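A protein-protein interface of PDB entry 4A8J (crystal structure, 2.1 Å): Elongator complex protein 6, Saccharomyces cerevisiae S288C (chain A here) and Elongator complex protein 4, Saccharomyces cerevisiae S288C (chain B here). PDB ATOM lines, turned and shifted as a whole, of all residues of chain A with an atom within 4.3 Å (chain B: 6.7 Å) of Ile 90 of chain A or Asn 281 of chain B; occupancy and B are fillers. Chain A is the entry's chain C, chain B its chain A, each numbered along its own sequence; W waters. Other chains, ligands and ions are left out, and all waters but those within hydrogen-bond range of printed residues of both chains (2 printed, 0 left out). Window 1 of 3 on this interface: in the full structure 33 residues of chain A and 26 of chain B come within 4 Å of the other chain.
A ring nitrogen (NE2) of His 247 of chain B lies within hydrogen-bond range of the backbone carbonyl oxygen (O) of Phe 89 of chain A, at 2.7 Å.
OD1 of Asn 281 of chain B sits at hydrogen-bond distance from ND2 of Asn 193 of chain A, 3.5 Å away.
The guanidinium group (NE) of Arg 250 of chain B sits at hydrogen-bond distance from the backbone carbonyl oxygen (O) of Ile 90 of chain A (2.8 Å).
The side-chain amide nitrogen (ND2) of Asn 281 of chain B is in hydrogen-bond range of the side-chain amide oxygen (OE1) of Gln 157 of chain A.
N of His 91 of chain A is in hydrogen-bond range of OG of Ser 88 of chain A (3.0 Å).
OD1 of Asp 284 of chain B is in salt-bridge range of NH1 of Arg 250 of chain B (3.1 Å).
OE1 of Glu 156 of chain A sits at hydrogen-bond distance from ND1 of His 91 of chain A.
The backbone NH of Ile 90 of chain A is in hydrogen-bond range of the side-chain hydroxyl of Ser 88 of chain A, 3.2 Å away.
The backbone carbonyl oxygen (O) of Glu 156 of chain A sits at hydrogen-bond distance from the backbone NH (N) of Phe 89 of chain A (3.1 Å).
The backbone carbonyl oxygen (O) of Met 282 of chain B lies within hydrogen-bond range of the guanidinium group (NH1) of Arg 250 of chain B (3.4 Å).
Among the printed residues, pairs that only touch across the chains: Ile 90 of chain A with Asn 281 of chain B (3.9 Å), Ile 90 of chain A with Met 282 of chain B (3.5 Å), His 91 of chain A with Arg 250 of chain B (3.4 Å), Leu 116 of chain A with His 247 of chain B (3.5 Å), Leu 116 of chain A with Lys 254 of chain B (3.95 Å), Leu 160 of chain A with Asn 281 of chain B (3.8 Å) and Leu 160 of chain A with Met 282 of chain B (3.9 Å).
Ile 90 of chain A touches three residues of chain B.
Printed residues of chain B within 4 Å of His 91 of chain A: Arg 250 (3.4 Å).
Printed residues of chain A within 4 Å of His 247 of chain B: Phe 89 (2.7 Å) and Leu 116 (3.5 Å).
Of chain A, only Ile 90 (3.9 Å), Gln 157 (2.8 Å), Leu 160 (3.8 Å) and Asn 193 (3.5 Å) come within 4 Å of Asn 281 of chain B.
The nearest printed residue of chain A that does not touch Lys 254 of chain B is Ile 90 of chain A (5.8 Å).
Of the 14 printed residues of chain B, 5 touch a printed residue of chain A.
Printed residues of chain B that touch a printed residue of chain A: His 247, Arg 250, Lys 254, Asn 281 and Met 282.
Hydrophobic or aromatic side chains of chain B that line the printed part of chain A: His 247 and Met 282.
Among the printed residues, 11 pairs touch across the chains.
Water W1 lies within hydrogen-bond range of a ring nitrogen (ND1) of His 247 of chain B and the backbone carbonyl oxygen of Leu 116 of chain A.
Water W2 lies within hydrogen-bond range of OD1 of Asn 281 of chain B (2.9 Å), ND2 of Asn 193 of chain A (3.1 Å) and NE2 of Gln 157 of chain A (3.1 Å).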
ATOM      1  N   SER A  88       2.742   8.531 -27.545  1.00  0.00           N
ATOM      2  CA  SER A  88       4.011   8.489 -26.813  1.00  0.00           C
ATOM      3  C   SER A  88       3.832   7.941 -25.402  1.00  0.00           C
ATOM      4  O   SER A  88       2.821   8.213 -24.754  1.00  0.00           O
ATOM      5  CB  SER A  88       4.662   9.883 -26.764  1.00  0.00           C
ATOM      6  OG  SER A  88       5.944   9.826 -26.158  1.00  0.00           O
ATOM      7  N   PHE A  89       4.813   7.164 -24.945  1.00  0.00           N
ATOM      8  CA  PHE A  89       4.862   6.698 -23.555  1.00  0.00           C
ATOM      9  C   PHE A  89       5.780   7.542 -22.683  1.00  0.00           C
ATOM     10  O   PHE A  89       5.944   7.255 -21.504  1.00  0.00           O
ATOM     11  CB  PHE A  89       5.253   5.208 -23.506  1.00  0.00           C
ATOM     12  CG  PHE A  89       4.205   4.307 -24.108  1.00  0.00           C
ATOM     13  CD1 PHE A  89       4.125   4.129 -25.476  1.00  0.00           C
ATOM     14  CD2 PHE A  89       3.258   3.691 -23.303  1.00  0.00           C
ATOM     15  CE1 PHE A  89       3.138   3.321 -26.036  1.00  0.00           C
ATOM     16  CE2 PHE A  89       2.268   2.883 -23.856  1.00  0.00           C
ATOM     17  CZ  PHE A  89       2.210   2.709 -25.223  1.00  0.00           C
ATOM     18  N   ILE A  90       6.368   8.587 -23.255  1.00  0.00           N
ATOM     19  CA  ILE A  90       7.339   9.423 -22.536  1.00  0.00           C
ATOM     20  C   ILE A  90       7.040  10.939 -22.633  1.00  0.00           C
ATOM     21  O   ILE A  90       7.479  11.722 -21.779  1.00  0.00           O
ATOM     22  CB  ILE A  90       8.781   9.147 -23.033  1.00  0.00           C
ATOM     23  CG1 ILE A  90       9.820   9.682 -22.047  1.00  0.00           C
ATOM     24  CG2 ILE A  90       8.995   9.719 -24.445  1.00  0.00           C
ATOM     25  CD1 ILE A  90       9.694   9.076 -20.644  1.00  0.00           C
ATOM     26  N   HIS A  91       6.289  11.355 -23.656  1.00  0.00           N
ATOM     27  CA  HIS A  91       5.893  12.772 -23.788  1.00  0.00           C
ATOM     28  C   HIS A  91       4.384  13.004 -23.691  1.00  0.00           C
ATOM     29  O   HIS A  91       3.599  12.250 -24.262  1.00  0.00           O
ATOM     30  CB  HIS A  91       6.423  13.368 -25.105  1.00  0.00           C
ATOM     31  CG  HIS A  91       7.909  13.537 -25.121  1.00  0.00           C
ATOM     32  ND1 HIS A  91       8.729  12.867 -26.003  1.00  0.00           N
ATOM     33  CD2 HIS A  91       8.728  14.270 -24.326  1.00  0.00           C
ATOM     34  CE1 HIS A  91       9.991  13.193 -25.764  1.00  0.00           C
ATOM     35  NE2 HIS A  91      10.015  14.046 -24.755  1.00  0.00           N
ATOM     36  N   LEU A 116       1.613   9.082 -21.284  1.00  0.00           N
ATOM     37  CA  LEU A 116       2.373   9.542 -20.114  1.00  0.00           C
ATOM     38  C   LEU A 116       1.386   9.997 -19.042  1.00  0.00           C
ATOM     39  O   LEU A 116       1.435   9.553 -17.908  1.00  0.00           O
ATOM     40  CB  LEU A 116       3.316  10.721 -20.477  1.00  0.00           C
ATOM     41  CG  LEU A 116       4.013  11.361 -19.262  1.00  0.00           C
ATOM     42  CD1 LEU A 116       4.960  10.392 -18.583  1.00  0.00           C
ATOM     43  CD2 LEU A 116       4.772  12.607 -19.675  1.00  0.00           C
ATOM     44  N   GLU A 156       5.937   6.292 -29.959  1.00  0.00           N
ATOM     45  CA  GLU A 156       7.230   6.597 -29.369  1.00  0.00           C
ATOM     46  C   GLU A 156       7.488   5.895 -28.036  1.00  0.00           C
ATOM     47  O   GLU A 156       6.706   6.013 -27.085  1.00  0.00           O
ATOM     48  CB  GLU A 156       7.379   8.111 -29.212  1.00  0.00           C
ATOM     49  CG  GLU A 156       8.619   8.526 -28.436  1.00  0.00           C
ATOM     50  CD  GLU A 156       8.772  10.055 -28.360  1.00  0.00           C
ATOM     51  OE1 GLU A 156       7.814  10.727 -27.919  1.00  0.00           O
ATOM     52  OE2 GLU A 156       9.843  10.579 -28.745  1.00  0.00           O
ATOM     53  N   GLN A 157       8.594   5.158 -27.994  1.00  0.00           N
ATOM     54  CA  GLN A 157       9.037   4.392 -26.816  1.00  0.00           C
ATOM     55  C   GLN A 157       8.035   3.397 -26.193  1.00  0.00           C
ATOM     56  O   GLN A 157       7.884   3.335 -24.964  1.00  0.00           O
ATOM     57  CB  GLN A 157       9.619   5.332 -25.746  1.00  0.00           C
ATOM     58  CG  GLN A 157      10.940   5.972 -26.175  1.00  0.00           C
ATOM     59  CD  GLN A 157      11.665   6.645 -25.028  1.00  0.00           C
ATOM     60  OE1 GLN A 157      11.730   6.103 -23.928  1.00  0.00           O
ATOM     61  NE2 GLN A 157      12.196   7.844 -25.274  1.00  0.00           N
ATOM     62  N   LEU A 160       8.967   1.054 -23.304  1.00  0.00           N
ATOM     63  CA  LEU A 160       8.911   1.465 -21.907  1.00  0.00           C
ATOM     64  C   LEU A 160       7.932   0.569 -21.152  1.00  0.00           C
ATOM     65  O   LEU A 160       8.042   0.419 -19.945  1.00  0.00           O
ATOM     66  CB  LEU A 160       8.526   2.939 -21.757  1.00  0.00           C
ATOM     67  CG  LEU A 160       9.694   3.925 -21.851  1.00  0.00           C
ATOM     68  CD1 LEU A 160       9.190   5.367 -21.757  1.00  0.00           C
ATOM     69  CD2 LEU A 160      10.729   3.680 -20.743  1.00  0.00           C
ATOM     70  N   ASN A 193      14.405   4.297 -28.039  1.00  0.00           N
ATOM     71  CA  ASN A 193      15.655   4.836 -27.518  1.00  0.00           C
ATOM     72  C   ASN A 193      16.687   3.732 -27.338  1.00  0.00           C
ATOM     73  O   ASN A 193      16.467   2.792 -26.589  1.00  0.00           O
ATOM     74  CB  ASN A 193      15.349   5.502 -26.166  1.00  0.00           C
ATOM     75  CG  ASN A 193      16.582   6.032 -25.474  1.00  0.00           C
ATOM     76  OD1 ASN A 193      17.667   5.469 -25.587  1.00  0.00           O
ATOM     77  ND2 ASN A 193      16.420   7.130 -24.741  1.00  0.00           N
ATOM     78  N   HIS B 247       7.860   7.674 -13.590  1.00  0.00           N
ATOM     79  CA  HIS B 247       7.014   7.979 -14.753  1.00  0.00           C
ATOM     80  C   HIS B 247       5.799   8.741 -14.248  1.00  0.00           C
ATOM     81  O   HIS B 247       5.437   9.791 -14.790  1.00  0.00           O
ATOM     82  CB  HIS B 247       6.612   6.674 -15.426  1.00  0.00           C
ATOM     83  CG  HIS B 247       5.904   6.839 -16.757  1.00  0.00           C
ATOM     84  ND1 HIS B 247       4.546   6.893 -16.859  1.00  0.00           N
ATOM     85  CD2 HIS B 247       6.400   6.870 -18.021  1.00  0.00           C
ATOM     86  CE1 HIS B 247       4.200   6.964 -18.152  1.00  0.00           C
ATOM     87  NE2 HIS B 247       5.313   6.956 -18.866  1.00  0.00           N
ATOM     88  N   ARG B 250       6.906  12.156 -13.419  1.00  0.00           N
ATOM     89  CA  ARG B 250       7.108  12.915 -14.637  1.00  0.00           C
ATOM     90  C   ARG B 250       5.712  13.337 -15.123  1.00  0.00           C
ATOM     91  O   ARG B 250       5.513  14.484 -15.540  1.00  0.00           O
ATOM     92  CB  ARG B 250       7.819  12.052 -15.703  1.00  0.00           C
ATOM     93  CG  ARG B 250       7.910  12.717 -17.091  1.00  0.00           C
ATOM     94  CD  ARG B 250       8.838  11.905 -17.986  1.00  0.00           C
ATOM     95  NE  ARG B 250       8.805  12.396 -19.361  1.00  0.00           N
ATOM     96  CZ  ARG B 250       9.575  13.371 -19.825  1.00  0.00           C
ATOM     97  NH1 ARG B 250      10.468  13.952 -19.024  1.00  0.00           N
ATOM     98  NH2 ARG B 250       9.460  13.751 -21.086  1.00  0.00           N
ATOM     99  N   LYS B 254       4.607  17.295 -15.868  1.00  0.00           N
ATOM    100  CA  LYS B 254       4.135  17.773 -17.184  1.00  0.00           C
ATOM    101  C   LYS B 254       2.673  18.219 -17.133  1.00  0.00           C
ATOM    102  O   LYS B 254       2.234  19.031 -17.935  1.00  0.00           O
ATOM    103  CB  LYS B 254       4.304  16.700 -18.269  1.00  0.00           C
ATOM    104  CG  LYS B 254       5.750  16.262 -18.536  1.00  0.00           C
ATOM    105  CD  LYS B 254       6.664  17.442 -18.789  1.00  0.00           C
ATOM    106  CE  LYS B 254       8.125  16.996 -18.905  1.00  0.00           C
ATOM    107  NZ  LYS B 254       9.021  18.133 -19.290  1.00  0.00           N
ATOM    108  N   LEU B 276      20.074   2.781 -14.361  1.00  0.00           N
ATOM    109  CA  LEU B 276      20.555   4.141 -14.554  1.00  0.00           C
ATOM    110  C   LEU B 276      20.085   4.710 -15.914  1.00  0.00           C
ATOM    111  O   LEU B 276      19.631   5.870 -15.990  1.00  0.00           O
ATOM    112  CB  LEU B 276      22.081   4.187 -14.444  1.00  0.00           C
ATOM    113  CG  LEU B 276      22.668   5.588 -14.590  1.00  0.00           C
ATOM    114  CD1 LEU B 276      22.019   6.539 -13.585  1.00  0.00           C
ATOM    115  CD2 LEU B 276      24.180   5.544 -14.422  1.00  0.00           C
ATOM    116  N   VAL B 277      20.197   3.933 -16.988  1.00  0.00           N
ATOM    117  CA  VAL B 277      19.694   4.472 -18.262  1.00  0.00           C
ATOM    118  C   VAL B 277      18.190   4.767 -18.206  1.00  0.00           C
ATOM    119  O   VAL B 277      17.763   5.777 -18.735  1.00  0.00           O
ATOM    120  CB  VAL B 277      20.022   3.636 -19.551  1.00  0.00           C
ATOM    121  CG1 VAL B 277      21.402   3.045 -19.495  1.00  0.00           C
ATOM    122  CG2 VAL B 277      18.987   2.580 -19.783  1.00  0.00           C
ATOM    123  N   LEU B 278      17.388   3.899 -17.586  1.00  0.00           N
ATOM    124  CA  LEU B 278      15.949   4.198 -17.471  1.00  0.00           C
ATOM    125  C   LEU B 278      15.688   5.466 -16.652  1.00  0.00           C
ATOM    126  O   LEU B 278      14.825   6.277 -16.998  1.00  0.00           O
ATOM    127  CB  LEU B 278      15.188   3.018 -16.847  1.00  0.00           C
ATOM    128  CG  LEU B 278      14.957   1.750 -17.670  1.00  0.00           C
ATOM    129  CD1 LEU B 278      14.616   0.570 -16.734  1.00  0.00           C
ATOM    130  CD2 LEU B 278      13.846   1.977 -18.715  1.00  0.00           C
ATOM    131  N   LEU B 279      16.427   5.641 -15.556  1.00  0.00           N
ATOM    132  CA  LEU B 279      16.231   6.820 -14.711  1.00  0.00           C
ATOM    133  C   LEU B 279      16.567   8.092 -15.480  1.00  0.00           C
ATOM    134  O   LEU B 279      15.840   9.077 -15.400  1.00  0.00           O
ATOM    135  CB  LEU B 279      17.082   6.749 -13.435  1.00  0.00           C
ATOM    136  CG  LEU B 279      16.617   5.737 -12.383  1.00  0.00           C
ATOM    137  CD1 LEU B 279      17.716   5.495 -11.318  1.00  0.00           C
ATOM    138  CD2 LEU B 279      15.339   6.262 -11.721  1.00  0.00           C
ATOM    139  N   ARG B 280      17.675   8.086 -16.212  1.00  0.00           N
ATOM    140  CA  ARG B 280      18.049   9.278 -16.967  1.00  0.00           C
ATOM    141  C   ARG B 280      16.939   9.621 -17.948  1.00  0.00           C
ATOM    142  O   ARG B 280      16.630  10.791 -18.178  1.00  0.00           O
ATOM    143  CB  ARG B 280      19.360   9.035 -17.718  1.00  0.00           C
ATOM    144  CG  ARG B 280      20.602   9.085 -16.816  1.00  0.00           C
ATOM    145  CD  ARG B 280      21.873   8.775 -17.598  1.00  0.00           C
ATOM    146  NE  ARG B 280      23.070   8.970 -16.765  1.00  0.00           N
ATOM    147  CZ  ARG B 280      24.255   8.417 -17.006  1.00  0.00           C
ATOM    148  NH1 ARG B 280      24.417   7.617 -18.052  1.00  0.00           N
ATOM    149  NH2 ARG B 280      25.276   8.663 -16.199  1.00  0.00           N
ATOM    150  N   ASN B 281      16.345   8.582 -18.533  1.00  0.00           N
ATOM    151  CA  ASN B 281      15.272   8.745 -19.512  1.00  0.00           C
ATOM    152  C   ASN B 281      14.036   9.452 -18.934  1.00  0.00           C
ATOM    153  O   ASN B 281      13.286  10.103 -19.672  1.00  0.00           O
ATOM    154  CB  ASN B 281      14.879   7.371 -20.090  1.00  0.00           C
ATOM    155  CG  ASN B 281      14.081   7.476 -21.396  1.00  0.00           C
ATOM    156  OD1 ASN B 281      14.337   8.333 -22.267  1.00  0.00           O
ATOM    157  ND2 ASN B 281      13.099   6.588 -21.533  1.00  0.00           N
ATOM    158  N   MET B 282      13.827   9.352 -17.619  1.00  0.00           N
ATOM    159  CA  MET B 282      12.667  10.009 -16.988  1.00  0.00           C
ATOM    160  C   MET B 282      12.874  11.507 -16.734  1.00  0.00           C
ATOM    161  O   MET B 282      11.918  12.235 -16.512  1.00  0.00           O
ATOM    162  CB  MET B 282      12.284   9.320 -15.665  1.00  0.00           C
ATOM    163  CG  MET B 282      11.858   7.863 -15.792  1.00  0.00           C
ATOM    164  SD  MET B 282      10.278   7.615 -16.930  1.00  0.00           S
ATOM    165  CE  MET B 282      11.157   6.783 -18.500  1.00  0.00           C
ATOM    166  N   PHE B 283      14.118  11.966 -16.745  1.00  0.00           N
ATOM    167  CA  PHE B 283      14.418  13.354 -16.411  1.00  0.00           C
ATOM    168  C   PHE B 283      14.735  14.241 -17.617  1.00  0.00           C
ATOM    169  O   PHE B 283      15.310  13.777 -18.600  1.00  0.00           O
ATOM    170  CB  PHE B 283      15.590  13.412 -15.418  1.00  0.00           C
ATOM    171  CG  PHE B 283      15.214  12.992 -14.033  1.00  0.00           C
ATOM    172  CD1 PHE B 283      15.082  11.643 -13.715  1.00  0.00           C
ATOM    173  CD2 PHE B 283      14.961  13.939 -13.058  1.00  0.00           C
ATOM    174  CE1 PHE B 283      14.717  11.240 -12.419  1.00  0.00           C
ATOM    175  CE2 PHE B 283      14.600  13.557 -11.763  1.00  0.00           C
ATOM    176  CZ  PHE B 283      14.468  12.203 -11.446  1.00  0.00           C
ATOM    177  N   ASP B 284      14.379  15.525 -17.521  1.00  0.00           N
ATOM    178  CA  ASP B 284      14.594  16.469 -18.617  1.00  0.00           C
ATOM    179  C   ASP B 284      16.042  16.931 -18.694  1.00  0.00           C
ATOM    180  O   ASP B 284      16.527  17.291 -19.762  1.00  0.00           O
ATOM    181  CB  ASP B 284      13.681  17.686 -18.442  1.00  0.00           C
ATOM    182  CG  ASP B 284      12.217  17.287 -18.286  1.00  0.00           C
ATOM    183  OD1 ASP B 284      11.615  16.869 -19.292  1.00  0.00           O
ATOM    184  OD2 ASP B 284      11.674  17.380 -17.157  1.00  0.00           O
ATOM    185  N   VAL B 286      20.162  16.193 -16.892  1.00  0.00           N
ATOM    186  CA  VAL B 286      21.019  15.347 -16.073  1.00  0.00           C
ATOM    187  C   VAL B 286      22.399  15.974 -15.973  1.00  0.00           C
ATOM    188  O   VAL B 286      23.033  16.309 -16.985  1.00  0.00           O
ATOM    189  CB  VAL B 286      21.148  13.929 -16.672  1.00  0.00           C
ATOM    190  CG1 VAL B 286      22.140  13.076 -15.831  1.00  0.00           C
ATOM    191  CG2 VAL B 286      19.770  13.253 -16.802  1.00  0.00           C
ATOM    192  N   LYS B 320      22.540  16.201 -20.329  1.00  0.00           N
ATOM    193  CA  LYS B 320      21.212  16.415 -20.890  1.00  0.00           C
ATOM    194  C   LYS B 320      20.709  17.743 -20.336  1.00  0.00           C
ATOM    195  O   LYS B 320      20.869  18.031 -19.145  1.00  0.00           O
ATOM    196  CB  LYS B 320      20.344  15.255 -20.430  1.00  0.00           C
ATOM    197  CG  LYS B 320      18.994  15.100 -21.018  1.00  0.00           C
ATOM    198  CD  LYS B 320      18.540  13.668 -20.680  1.00  0.00           C
ATOM    199  CE  LYS B 320      17.071  13.450 -20.954  1.00  0.00           C
ATOM    200  NZ  LYS B 320      16.692  12.077 -20.536  1.00  0.00           N
HETATM  201  O   HOH W   1       2.373   7.981 -15.729  1.00  0.00           O
HETATM  202  O   HOH W   2      14.704   9.670 -24.864  1.00  0.00           O
